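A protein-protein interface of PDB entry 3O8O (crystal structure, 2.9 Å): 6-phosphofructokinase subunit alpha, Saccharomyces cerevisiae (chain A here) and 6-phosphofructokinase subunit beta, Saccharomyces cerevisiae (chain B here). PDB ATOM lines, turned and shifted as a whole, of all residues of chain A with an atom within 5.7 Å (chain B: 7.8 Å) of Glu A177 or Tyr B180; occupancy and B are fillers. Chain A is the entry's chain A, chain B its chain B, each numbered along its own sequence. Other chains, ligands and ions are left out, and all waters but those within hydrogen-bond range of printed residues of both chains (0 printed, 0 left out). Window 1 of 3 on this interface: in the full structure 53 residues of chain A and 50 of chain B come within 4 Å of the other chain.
Hydrophobic or aromatic side chains of chain B that line the printed part of chain A: Ala B177, Tyr B180, Phe B192 and Val B289. Of the 18 printed residues of chain A, 9 touch a printed residue of chain B. Among the printed residues, no Asp or Glu carboxylate lies within 4 Å of a Lys or Arg side-chain nitrogen of the other chain.
Of the printed residues of chain B, Arg A174 touches Tyr B180. Of chain B, only Tyr B180 comes within 4 Å of Glu A177. Of the printed residues of chain B, Tyr A181 touches Arg B173 (3.4 Å) and Gly B293 (3.1 Å). Printed residues of chain B within 4 Å of His A288: Thr B184 and Phe B192. Of the printed residues of chain B, Gly A292 touches Tyr B180. Tyr B180 touches just these residues of chain A: Arg A174 (3.4 Å), Glu A177 (2.7 Å), Val A289 (3.96 Å), Gly A292 (3.1 Å) and Gly A293 (3.2 Å). Val B181 touches none of the printed residues of chain A. Ala B185 touches none of the printed residues of chain A. Of the printed residues of chain A, Phe B192 touches His A288 (3.4 Å). The nearest printed residue of chain B that does not touch Arg A291 is Tyr B180 (4.9 Å).
Among the printed residues, merely in contact across the chains: Gly A292 with Tyr B180 (3.1 Å), Tyr A181 with Gly B293 (3.1 Å), Gly A293 with Tyr B180 (3.2 Å), Tyr A181 with Arg B173 (3.4 Å), His A288 with Phe B192 (3.4 Å), Arg A174 with Tyr B180 (3.4 Å), Met A178 with Val B289 (3.5 Å), Val A289 with Ala B177 (3.8 Å), His A288 with Thr B184 (3.9 Å) and Val A289 with Tyr B180 (3.96 Å).
The guanidinium group of Arg A174 is in hydrogen-bond range of the backbone carbonyl oxygen of Thr A294 (2.6 Å). The side-chain carboxylate (OE2) of Glu A177 is in hydrogen-bond range of the side-chain hydroxyl (OH) of Tyr A181 (3.0 Å). The side-chain carboxylate (OD2) of Asp B172 lies within salt-bridge range of the guanidinium group (NH1) of Arg B173, 2.9 Å away.
The side-chain carboxylate (OE1) of Glu A177 sits at hydrogen-bond distance from the side-chain hydroxyl (OH) of Tyr B180 (2.7 Å). The side-chain hydroxyl (OG1) of Thr B184 lies within hydrogen-bond range of the guanidinium group (NH2) of Arg A291, at 3.2 Å.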
ATOM      1  N   LEU A 172     -27.659  -4.397  36.611  1.00  0.00           N
ATOM      2  CA  LEU A 172     -27.445  -2.989  36.898  1.00  0.00           C
ATOM      3  C   LEU A 172     -25.961  -2.690  36.863  1.00  0.00           C
ATOM      4  O   LEU A 172     -25.521  -1.760  36.181  1.00  0.00           O
ATOM      5  CB  LEU A 172     -27.989  -2.628  38.264  1.00  0.00           C
ATOM      6  CG  LEU A 172     -27.763  -1.190  38.730  1.00  0.00           C
ATOM      7  CD1 LEU A 172     -28.213  -0.197  37.685  1.00  0.00           C
ATOM      8  CD2 LEU A 172     -28.565  -0.941  40.008  1.00  0.00           C
ATOM      9  N   GLU A 173     -25.184  -3.494  37.588  1.00  0.00           N
ATOM     10  CA  GLU A 173     -23.753  -3.291  37.613  1.00  0.00           C
ATOM     11  C   GLU A 173     -23.224  -3.271  36.189  1.00  0.00           C
ATOM     12  O   GLU A 173     -22.432  -2.403  35.831  1.00  0.00           O
ATOM     13  CB  GLU A 173     -23.072  -4.389  38.418  1.00  0.00           C
ATOM     14  CG  GLU A 173     -21.681  -3.988  38.916  1.00  0.00           C
ATOM     15  CD  GLU A 173     -21.679  -2.701  39.752  1.00  0.00           C
ATOM     16  OE1 GLU A 173     -20.674  -1.978  39.666  1.00  0.00           O
ATOM     17  OE2 GLU A 173     -22.652  -2.407  40.487  1.00  0.00           O
ATOM     18  N   ARG A 174     -23.679  -4.212  35.368  1.00  0.00           N
ATOM     19  CA  ARG A 174     -23.233  -4.258  33.983  1.00  0.00           C
ATOM     20  C   ARG A 174     -23.574  -2.968  33.217  1.00  0.00           C
ATOM     21  O   ARG A 174     -22.752  -2.445  32.447  1.00  0.00           O
ATOM     22  CB  ARG A 174     -23.829  -5.475  33.291  1.00  0.00           C
ATOM     23  CG  ARG A 174     -22.750  -6.332  32.687  1.00  0.00           C
ATOM     24  CD  ARG A 174     -21.813  -6.821  33.771  1.00  0.00           C
ATOM     25  NE  ARG A 174     -22.452  -7.877  34.544  1.00  0.00           N
ATOM     26  CZ  ARG A 174     -21.981  -8.376  35.679  1.00  0.00           C
ATOM     27  NH1 ARG A 174     -20.855  -7.908  36.200  1.00  0.00           N
ATOM     28  NH2 ARG A 174     -22.630  -9.362  36.281  1.00  0.00           N
ATOM     29  N   ILE A 175     -24.778  -2.450  33.432  1.00  0.00           N
ATOM     30  CA  ILE A 175     -25.157  -1.216  32.770  1.00  0.00           C
ATOM     31  C   ILE A 175     -24.159  -0.145  33.170  1.00  0.00           C
ATOM     32  O   ILE A 175     -23.544   0.494  32.309  1.00  0.00           O
ATOM     33  CB  ILE A 175     -26.557  -0.734  33.183  1.00  0.00           C
ATOM     34  CG1 ILE A 175     -27.606  -1.733  32.709  1.00  0.00           C
ATOM     35  CG2 ILE A 175     -26.838   0.638  32.607  1.00  0.00           C
ATOM     36  CD1 ILE A 175     -29.018  -1.406  33.216  1.00  0.00           C
ATOM     37  N   CYS A 176     -23.997   0.056  34.475  1.00  0.00           N
ATOM     38  CA  CYS A 176     -23.073   1.068  34.972  1.00  0.00           C
ATOM     39  C   CYS A 176     -21.716   0.947  34.299  1.00  0.00           C
ATOM     40  O   CYS A 176     -21.152   1.943  33.846  1.00  0.00           O
ATOM     41  CB  CYS A 176     -22.911   0.955  36.488  1.00  0.00           C
ATOM     42  SG  CYS A 176     -24.306   1.620  37.447  1.00  0.00           S
ATOM     43  N   GLU A 177     -21.208  -0.279  34.208  1.00  0.00           N
ATOM     44  CA  GLU A 177     -19.911  -0.497  33.587  1.00  0.00           C
ATOM     45  C   GLU A 177     -19.932   0.110  32.212  1.00  0.00           C
ATOM     46  O   GLU A 177     -19.181   1.027  31.932  1.00  0.00           O
ATOM     47  CB  GLU A 177     -19.571  -1.991  33.476  1.00  0.00           C
ATOM     48  CG  GLU A 177     -18.184  -2.249  32.876  1.00  0.00           C
ATOM     49  CD  GLU A 177     -17.833  -3.722  32.780  1.00  0.00           C
ATOM     50  OE1 GLU A 177     -18.340  -4.518  33.605  1.00  0.00           O
ATOM     51  OE2 GLU A 177     -17.038  -4.080  31.892  1.00  0.00           O
ATOM     52  N   MET A 178     -20.821  -0.391  31.361  1.00  0.00           N
ATOM     53  CA  MET A 178     -20.903   0.096  29.990  1.00  0.00           C
ATOM     54  C   MET A 178     -21.055   1.610  29.940  1.00  0.00           C
ATOM     55  O   MET A 178     -20.318   2.282  29.218  1.00  0.00           O
ATOM     56  CB  MET A 178     -22.054  -0.590  29.221  1.00  0.00           C
ATOM     57  CG  MET A 178     -22.021  -2.122  29.175  1.00  0.00           C
ATOM     58  SD  MET A 178     -20.407  -2.931  29.035  1.00  0.00           S
ATOM     59  CE  MET A 178     -20.034  -2.847  27.284  1.00  0.00           C
ATOM     60  N   VAL A 179     -21.988   2.160  30.707  1.00  0.00           N
ATOM     61  CA  VAL A 179     -22.152   3.606  30.671  1.00  0.00           C
ATOM     62  C   VAL A 179     -20.880   4.363  31.070  1.00  0.00           C
ATOM     63  O   VAL A 179     -20.555   5.394  30.475  1.00  0.00           O
ATOM     64  CB  VAL A 179     -23.318   4.076  31.561  1.00  0.00           C
ATOM     65  CG1 VAL A 179     -23.529   5.591  31.408  1.00  0.00           C
ATOM     66  CG2 VAL A 179     -24.571   3.345  31.172  1.00  0.00           C
ATOM     67  N   ASP A 180     -20.163   3.852  32.072  1.00  0.00           N
ATOM     68  CA  ASP A 180     -18.929   4.486  32.511  1.00  0.00           C
ATOM     69  C   ASP A 180     -17.968   4.559  31.339  1.00  0.00           C
ATOM     70  O   ASP A 180     -17.300   5.575  31.164  1.00  0.00           O
ATOM     71  CB  ASP A 180     -18.267   3.714  33.659  1.00  0.00           C
ATOM     72  CG  ASP A 180     -19.010   3.850  34.983  1.00  0.00           C
ATOM     73  OD1 ASP A 180     -19.821   4.809  35.153  1.00  0.00           O
ATOM     74  OD2 ASP A 180     -18.752   2.971  35.848  1.00  0.00           O
ATOM     75  N   TYR A 181     -17.884   3.494  30.544  1.00  0.00           N
ATOM     76  CA  TYR A 181     -16.992   3.495  29.369  1.00  0.00           C
ATOM     77  C   TYR A 181     -17.422   4.641  28.444  1.00  0.00           C
ATOM     78  O   TYR A 181     -16.631   5.530  28.093  1.00  0.00           O
ATOM     79  CB  TYR A 181     -17.110   2.198  28.562  1.00  0.00           C
ATOM     80  CG  TYR A 181     -16.496   0.957  29.167  1.00  0.00           C
ATOM     81  CD1 TYR A 181     -17.249  -0.219  29.308  1.00  0.00           C
ATOM     82  CD2 TYR A 181     -15.169   0.934  29.555  1.00  0.00           C
ATOM     83  CE1 TYR A 181     -16.695  -1.370  29.813  1.00  0.00           C
ATOM     84  CE2 TYR A 181     -14.603  -0.218  30.061  1.00  0.00           C
ATOM     85  CZ  TYR A 181     -15.375  -1.372  30.189  1.00  0.00           C
ATOM     86  OH  TYR A 181     -14.827  -2.532  30.695  1.00  0.00           O
ATOM     87  N   ILE A 182     -18.694   4.598  28.058  1.00  0.00           N
ATOM     88  CA  ILE A 182     -19.263   5.600  27.178  1.00  0.00           C
ATOM     89  C   ILE A 182     -18.908   7.005  27.642  1.00  0.00           C
ATOM     90  O   ILE A 182     -18.597   7.880  26.823  1.00  0.00           O
ATOM     91  CB  ILE A 182     -20.804   5.457  27.107  1.00  0.00           C
ATOM     92  CG1 ILE A 182     -21.171   4.125  26.440  1.00  0.00           C
ATOM     93  CG2 ILE A 182     -21.412   6.650  26.359  1.00  0.00           C
ATOM     94  CD1 ILE A 182     -22.662   3.832  26.450  1.00  0.00           C
ATOM     95  N   HIS A 288     -27.603  -7.681  25.367  1.00  0.00           N
ATOM     96  CA  HIS A 288     -27.370  -8.740  26.337  1.00  0.00           C
ATOM     97  C   HIS A 288     -26.178  -8.694  27.267  1.00  0.00           C
ATOM     98  O   HIS A 288     -26.021  -9.582  28.109  1.00  0.00           O
ATOM     99  CB  HIS A 288     -27.433 -10.088  25.626  1.00  0.00           C
ATOM    100  CG  HIS A 288     -28.786 -10.379  25.060  1.00  0.00           C
ATOM    101  ND1 HIS A 288     -29.244  -9.790  23.903  1.00  0.00           N
ATOM    102  CD2 HIS A 288     -29.831 -11.073  25.568  1.00  0.00           C
ATOM    103  CE1 HIS A 288     -30.513 -10.104  23.726  1.00  0.00           C
ATOM    104  NE2 HIS A 288     -30.893 -10.878  24.723  1.00  0.00           N
ATOM    105  N   VAL A 289     -25.334  -7.679  27.146  1.00  0.00           N
ATOM    106  CA  VAL A 289     -24.225  -7.601  28.069  1.00  0.00           C
ATOM    107  C   VAL A 289     -24.855  -7.535  29.463  1.00  0.00           C
ATOM    108  O   VAL A 289     -24.235  -7.883  30.469  1.00  0.00           O
ATOM    109  CB  VAL A 289     -23.399  -6.354  27.814  1.00  0.00           C
ATOM    110  CG1 VAL A 289     -22.439  -6.599  26.644  1.00  0.00           C
ATOM    111  CG2 VAL A 289     -24.330  -5.196  27.537  1.00  0.00           C
ATOM    112  N   ARG A 291     -26.994  -9.422  30.673  1.00  0.00           N
ATOM    113  CA  ARG A 291     -27.444 -10.741  31.104  1.00  0.00           C
ATOM    114  C   ARG A 291     -26.285 -11.657  31.433  1.00  0.00           C
ATOM    115  O   ARG A 291     -26.474 -12.685  32.089  1.00  0.00           O
ATOM    116  CB  ARG A 291     -28.277 -11.378  29.993  1.00  0.00           C
ATOM    117  CG  ARG A 291     -29.623 -10.729  29.760  1.00  0.00           C
ATOM    118  CD  ARG A 291     -30.680 -11.335  30.677  1.00  0.00           C
ATOM    119  NE  ARG A 291     -30.933 -12.740  30.349  1.00  0.00           N
ATOM    120  CZ  ARG A 291     -31.552 -13.150  29.248  1.00  0.00           C
ATOM    121  NH1 ARG A 291     -31.994 -12.263  28.366  1.00  0.00           N
ATOM    122  NH2 ARG A 291     -31.718 -14.445  29.026  1.00  0.00           N
ATOM    123  N   GLY A 292     -25.094 -11.290  30.957  1.00  0.00           N
ATOM    124  CA  GLY A 292     -23.911 -12.096  31.204  1.00  0.00           C
ATOM    125  C   GLY A 292     -23.153 -11.688  32.451  1.00  0.00           C
ATOM    126  O   GLY A 292     -23.684 -11.006  33.325  1.00  0.00           O
ATOM    127  N   GLY A 293     -21.903 -12.116  32.540  1.00  0.00           N
ATOM    128  CA  GLY A 293     -21.114 -11.756  33.698  1.00  0.00           C
ATOM    129  C   GLY A 293     -21.518 -12.592  34.883  1.00  0.00           C
ATOM    130  O   GLY A 293     -22.616 -13.152  34.892  1.00  0.00           O
ATOM    131  N   THR A 294     -20.637 -12.677  35.877  1.00  0.00           N
ATOM    132  CA  THR A 294     -20.917 -13.481  37.061  1.00  0.00           C
ATOM    133  C   THR A 294     -21.875 -12.691  37.920  1.00  0.00           C
ATOM    134  O   THR A 294     -22.256 -11.576  37.572  1.00  0.00           O
ATOM    135  CB  THR A 294     -19.645 -13.758  37.904  1.00  0.00           C
ATOM    136  OG1 THR A 294     -19.216 -12.533  38.505  1.00  0.00           O
ATOM    137  CG2 THR A 294     -18.518 -14.307  37.051  1.00  0.00           C
ATOM    138  N   ARG A 671     -23.454   3.835  44.790  1.00  0.00           N
ATOM    139  CA  ARG A 671     -23.732   5.106  44.139  1.00  0.00           C
ATOM    140  C   ARG A 671     -25.159   5.543  44.422  1.00  0.00           C
ATOM    141  O   ARG A 671     -25.397   6.718  44.690  1.00  0.00           O
ATOM    142  CB  ARG A 671     -23.543   5.030  42.626  1.00  0.00           C
ATOM    143  CG  ARG A 671     -22.190   4.580  42.162  1.00  0.00           C
ATOM    144  CD  ARG A 671     -22.148   4.723  40.667  1.00  0.00           C
ATOM    145  NE  ARG A 671     -21.142   3.875  40.041  1.00  0.00           N
ATOM    146  CZ  ARG A 671     -20.807   3.958  38.756  1.00  0.00           C
ATOM    147  NH1 ARG A 671     -21.396   4.851  37.978  1.00  0.00           N
ATOM    148  NH2 ARG A 671     -19.894   3.141  38.251  1.00  0.00           N
ATOM    149  N   ASP B 172     -10.037  -5.063  23.837  1.00  0.00           N
ATOM    150  CA  ASP B 172     -10.322  -5.492  25.217  1.00  0.00           C
ATOM    151  C   ASP B 172     -11.810  -5.269  25.501  1.00  0.00           C
ATOM    152  O   ASP B 172     -12.513  -6.140  25.998  1.00  0.00           O
ATOM    153  CB  ASP B 172      -9.482  -4.658  26.202  1.00  0.00           C
ATOM    154  CG  ASP B 172      -9.660  -5.090  27.653  1.00  0.00           C
ATOM    155  OD1 ASP B 172      -9.053  -6.111  28.072  1.00  0.00           O
ATOM    156  OD2 ASP B 172     -10.416  -4.397  28.369  1.00  0.00           O
ATOM    157  N   ARG B 173     -12.282  -4.081  25.177  1.00  0.00           N
ATOM    158  CA  ARG B 173     -13.673  -3.770  25.384  1.00  0.00           C
ATOM    159  C   ARG B 173     -14.568  -4.766  24.665  1.00  0.00           C
ATOM    160  O   ARG B 173     -15.568  -5.226  25.219  1.00  0.00           O
ATOM    161  CB  ARG B 173     -13.964  -2.347  24.898  1.00  0.00           C
ATOM    162  CG  ARG B 173     -14.430  -1.436  26.010  1.00  0.00           C
ATOM    163  CD  ARG B 173     -13.427  -1.451  27.162  1.00  0.00           C
ATOM    164  NE  ARG B 173     -12.453  -0.373  27.040  1.00  0.00           N
ATOM    165  CZ  ARG B 173     -11.217  -0.428  27.520  1.00  0.00           C
ATOM    166  NH1 ARG B 173     -10.801  -1.517  28.148  1.00  0.00           N
ATOM    167  NH2 ARG B 173     -10.408   0.612  27.391  1.00  0.00           N
ATOM    168  N   ILE B 174     -14.196  -5.099  23.427  1.00  0.00           N
ATOM    169  CA  ILE B 174     -14.965  -6.033  22.599  1.00  0.00           C
ATOM    170  C   ILE B 174     -15.045  -7.412  23.236  1.00  0.00           C
ATOM    171  O   ILE B 174     -16.133  -7.929  23.459  1.00  0.00           O
ATOM    172  CB  ILE B 174     -14.357  -6.158  21.150  1.00  0.00           C
ATOM    173  CG1 ILE B 174     -14.608  -4.858  20.365  1.00  0.00           C
ATOM    174  CG2 ILE B 174     -14.975  -7.349  20.408  1.00  0.00           C
ATOM    175  CD1 ILE B 174     -13.824  -4.727  19.082  1.00  0.00           C
ATOM    176  N   CYS B 175     -13.889  -7.986  23.541  1.00  0.00           N
ATOM    177  CA  CYS B 175     -13.823  -9.309  24.128  1.00  0.00           C
ATOM    178  C   CYS B 175     -14.531  -9.377  25.446  1.00  0.00           C
ATOM    179  O   CYS B 175     -14.985 -10.457  25.838  1.00  0.00           O
ATOM    180  CB  CYS B 175     -12.385  -9.741  24.330  1.00  0.00           C
ATOM    181  SG  CYS B 175     -11.462  -9.855  22.808  1.00  0.00           S
ATOM    182  N   LYS B 176     -14.630  -8.243  26.141  1.00  0.00           N
ATOM    183  CA  LYS B 176     -15.316  -8.228  27.430  1.00  0.00           C
ATOM    184  C   LYS B 176     -16.818  -8.315  27.206  1.00  0.00           C
ATOM    185  O   LYS B 176     -17.512  -9.025  27.921  1.00  0.00           O
ATOM    186  CB  LYS B 176     -14.933  -6.977  28.237  1.00  0.00           C
ATOM    187  N   ALA B 177     -17.307  -7.618  26.186  1.00  0.00           N
ATOM    188  CA  ALA B 177     -18.727  -7.640  25.887  1.00  0.00           C
ATOM    189  C   ALA B 177     -19.130  -9.020  25.375  1.00  0.00           C
ATOM    190  O   ALA B 177     -20.151  -9.577  25.780  1.00  0.00           O
ATOM    191  CB  ALA B 177     -19.045  -6.587  24.866  1.00  0.00           C
ATOM    192  N   ILE B 178     -18.328  -9.579  24.484  1.00  0.00           N
ATOM    193  CA  ILE B 178     -18.645 -10.884  23.958  1.00  0.00           C
ATOM    194  C   ILE B 178     -18.645 -11.874  25.096  1.00  0.00           C
ATOM    195  O   ILE B 178     -19.543 -12.708  25.157  1.00  0.00           O
ATOM    196  CB  ILE B 178     -17.646 -11.299  22.847  1.00  0.00           C
ATOM    197  CG1 ILE B 178     -17.930 -10.452  21.601  1.00  0.00           C
ATOM    198  CG2 ILE B 178     -17.734 -12.795  22.536  1.00  0.00           C
ATOM    199  CD1 ILE B 178     -16.875 -10.573  20.520  1.00  0.00           C
ATOM    200  N   ASP B 179     -17.679 -11.786  26.013  1.00  0.00           N
ATOM    201  CA  ASP B 179     -17.659 -12.743  27.126  1.00  0.00           C
ATOM    202  C   ASP B 179     -18.925 -12.654  27.971  1.00  0.00           C
ATOM    203  O   ASP B 179     -19.317 -13.621  28.606  1.00  0.00           O
ATOM    204  CB  ASP B 179     -16.450 -12.557  28.044  1.00  0.00           C
ATOM    205  N   TYR B 180     -19.561 -11.493  27.995  1.00  0.00           N
ATOM    206  CA  TYR B 180     -20.782 -11.363  28.765  1.00  0.00           C
ATOM    207  C   TYR B 180     -21.896 -12.036  27.974  1.00  0.00           C
ATOM    208  O   TYR B 180     -22.620 -12.887  28.499  1.00  0.00           O
ATOM    209  CB  TYR B 180     -21.131  -9.896  28.982  1.00  0.00           C
ATOM    210  CG  TYR B 180     -20.326  -9.206  30.050  1.00  0.00           C
ATOM    211  CD1 TYR B 180     -20.189  -9.767  31.318  1.00  0.00           C
ATOM    212  CD2 TYR B 180     -19.782  -7.944  29.828  1.00  0.00           C
ATOM    213  CE1 TYR B 180     -19.543  -9.086  32.338  1.00  0.00           C
ATOM    214  CE2 TYR B 180     -19.134  -7.256  30.842  1.00  0.00           C
ATOM    215  CZ  TYR B 180     -19.024  -7.834  32.091  1.00  0.00           C
ATOM    216  OH  TYR B 180     -18.416  -7.136  33.090  1.00  0.00           O
ATOM    217  N   VAL B 181     -22.024 -11.640  26.708  1.00  0.00           N
ATOM    218  CA  VAL B 181     -23.042 -12.189  25.811  1.00  0.00           C
ATOM    219  C   VAL B 181     -23.002 -13.713  25.798  1.00  0.00           C
ATOM    220  O   VAL B 181     -24.038 -14.379  25.859  1.00  0.00           O
ATOM    221  CB  VAL B 181     -22.836 -11.673  24.369  1.00  0.00           C
ATOM    222  CG1 VAL B 181     -23.667 -12.480  23.399  1.00  0.00           C
ATOM    223  CG2 VAL B 181     -23.228 -10.215  24.293  1.00  0.00           C
ATOM    224  N   GLU B 182     -21.792 -14.251  25.732  1.00  0.00           N
ATOM    225  CA  GLU B 182     -21.596 -15.681  25.693  1.00  0.00           C
ATOM    226  C   GLU B 182     -22.297 -16.428  26.813  1.00  0.00           C
ATOM    227  O   GLU B 182     -22.802 -17.521  26.590  1.00  0.00           O
ATOM    228  CB  GLU B 182     -20.121 -16.009  25.755  1.00  0.00           C
ATOM    229  CG  GLU B 182     -19.819 -17.461  25.529  1.00  0.00           C
ATOM    230  CD  GLU B 182     -19.440 -17.729  24.108  1.00  0.00           C
ATOM    231  OE1 GLU B 182     -18.518 -17.048  23.611  1.00  0.00           O
ATOM    232  OE2 GLU B 182     -20.054 -18.616  23.483  1.00  0.00           O
ATOM    233  N   ALA B 183     -22.334 -15.861  28.013  1.00  0.00           N
ATOM    234  CA  ALA B 183     -22.978 -16.545  29.138  1.00  0.00           C
ATOM    235  C   ALA B 183     -24.485 -16.656  29.032  1.00  0.00           C
ATOM    236  O   ALA B 183     -25.059 -17.674  29.415  1.00  0.00           O
ATOM    237  CB  ALA B 183     -22.611 -15.871  30.452  1.00  0.00           C
ATOM    238  N   THR B 184     -25.149 -15.620  28.542  1.00  0.00           N
ATOM    239  CA  THR B 184     -26.589 -15.735  28.438  1.00  0.00           C
ATOM    240  C   THR B 184     -26.879 -16.579  27.187  1.00  0.00           C
ATOM    241  O   THR B 184     -27.849 -17.352  27.140  1.00  0.00           O
ATOM    242  CB  THR B 184     -27.221 -14.365  28.359  1.00  0.00           C
ATOM    243  OG1 THR B 184     -28.650 -14.500  28.264  1.00  0.00           O
ATOM    244  CG2 THR B 184     -26.610 -13.590  27.193  1.00  0.00           C
ATOM    245  N   ALA B 185     -25.998 -16.458  26.195  1.00  0.00           N
ATOM    246  CA  ALA B 185     -26.127 -17.229  24.965  1.00  0.00           C
ATOM    247  C   ALA B 185     -26.076 -18.704  25.299  1.00  0.00           C
ATOM    248  O   ALA B 185     -26.852 -19.485  24.790  1.00  0.00           O
ATOM    249  CB  ALA B 185     -25.008 -16.898  24.005  1.00  0.00           C
ATOM    250  N   ASN B 186     -25.144 -19.085  26.154  1.00  0.00           N
ATOM    251  CA  ASN B 186     -24.994 -20.478  26.567  1.00  0.00           C
ATOM    252  C   ASN B 186     -26.211 -20.997  27.349  1.00  0.00           C
ATOM    253  O   ASN B 186     -26.502 -22.186  27.337  1.00  0.00           O
ATOM    254  CB  ASN B 186     -23.751 -20.609  27.435  1.00  0.00           C
ATOM    255  CG  ASN B 186     -23.413 -22.038  27.750  1.00  0.00           C
ATOM    256  OD1 ASN B 186     -22.607 -22.656  27.061  1.00  0.00           O
ATOM    257  ND2 ASN B 186     -24.034 -22.581  28.792  1.00  0.00           N
ATOM    258  N   PHE B 192     -25.622 -15.301  18.401  1.00  0.00           N
ATOM    259  CA  PHE B 192     -25.537 -13.852  18.437  1.00  0.00           C
ATOM    260  C   PHE B 192     -24.647 -13.344  17.311  1.00  0.00           C
ATOM    261  O   PHE B 192     -23.589 -13.918  17.000  1.00  0.00           O
ATOM    262  CB  PHE B 192     -24.957 -13.365  19.783  1.00  0.00           C
ATOM    263  CG  PHE B 192     -25.940 -13.382  20.940  1.00  0.00           C
ATOM    264  CD1 PHE B 192     -26.032 -14.486  21.787  1.00  0.00           C
ATOM    265  CD2 PHE B 192     -26.763 -12.283  21.183  1.00  0.00           C
ATOM    266  CE1 PHE B 192     -26.929 -14.491  22.850  1.00  0.00           C
ATOM    267  CE2 PHE B 192     -27.662 -12.282  22.250  1.00  0.00           C
ATOM    268  CZ  PHE B 192     -27.745 -13.385  23.081  1.00  0.00           C
ATOM    269  N   VAL B 289     -18.969   1.756  23.361  1.00  0.00           N
ATOM    270  CA  VAL B 289     -18.308   1.275  24.572  1.00  0.00           C
ATOM    271  C   VAL B 289     -16.919   0.855  24.106  1.00  0.00           C
ATOM    272  O   VAL B 289     -15.993   0.738  24.893  1.00  0.00           O
ATOM    273  CB  VAL B 289     -19.003   0.036  25.238  1.00  0.00           C
ATOM    274  CG1 VAL B 289     -20.501   0.260  25.389  1.00  0.00           C
ATOM    275  CG2 VAL B 289     -18.701  -1.214  24.461  1.00  0.00           C
ATOM    276  N   GLY B 293     -13.628   3.586  28.249  1.00  0.00           N
ATOM    277  CA  GLY B 293     -12.746   2.815  29.093  1.00  0.00           C
ATOM    278  C   GLY B 293     -11.346   3.399  29.172  1.00  0.00           C
ATOM    279  O   GLY B 293     -10.934   4.205  28.336  1.00  0.00           O
ATOM    280  N   LEU B 666      -9.546 -13.488  33.719  1.00  0.00           N
ATOM    281  CA  LEU B 666      -9.698 -13.875  32.318  1.00  0.00           C
ATOM    282  C   LEU B 666      -8.530 -13.336  31.534  1.00  0.00           C
ATOM    283  O   LEU B 666      -8.281 -12.141  31.541  1.00  0.00           O
ATOM    284  CB  LEU B 666     -10.985 -13.286  31.764  1.00  0.00           C
ATOM    285  CG  LEU B 666     -12.220 -13.831  32.501  1.00  0.00           C
ATOM    286  CD1 LEU B 666     -13.492 -13.177  31.995  1.00  0.00           C
ATOM    287  CD2 LEU B 666     -12.250 -15.399  32.372  1.00  0.00           C
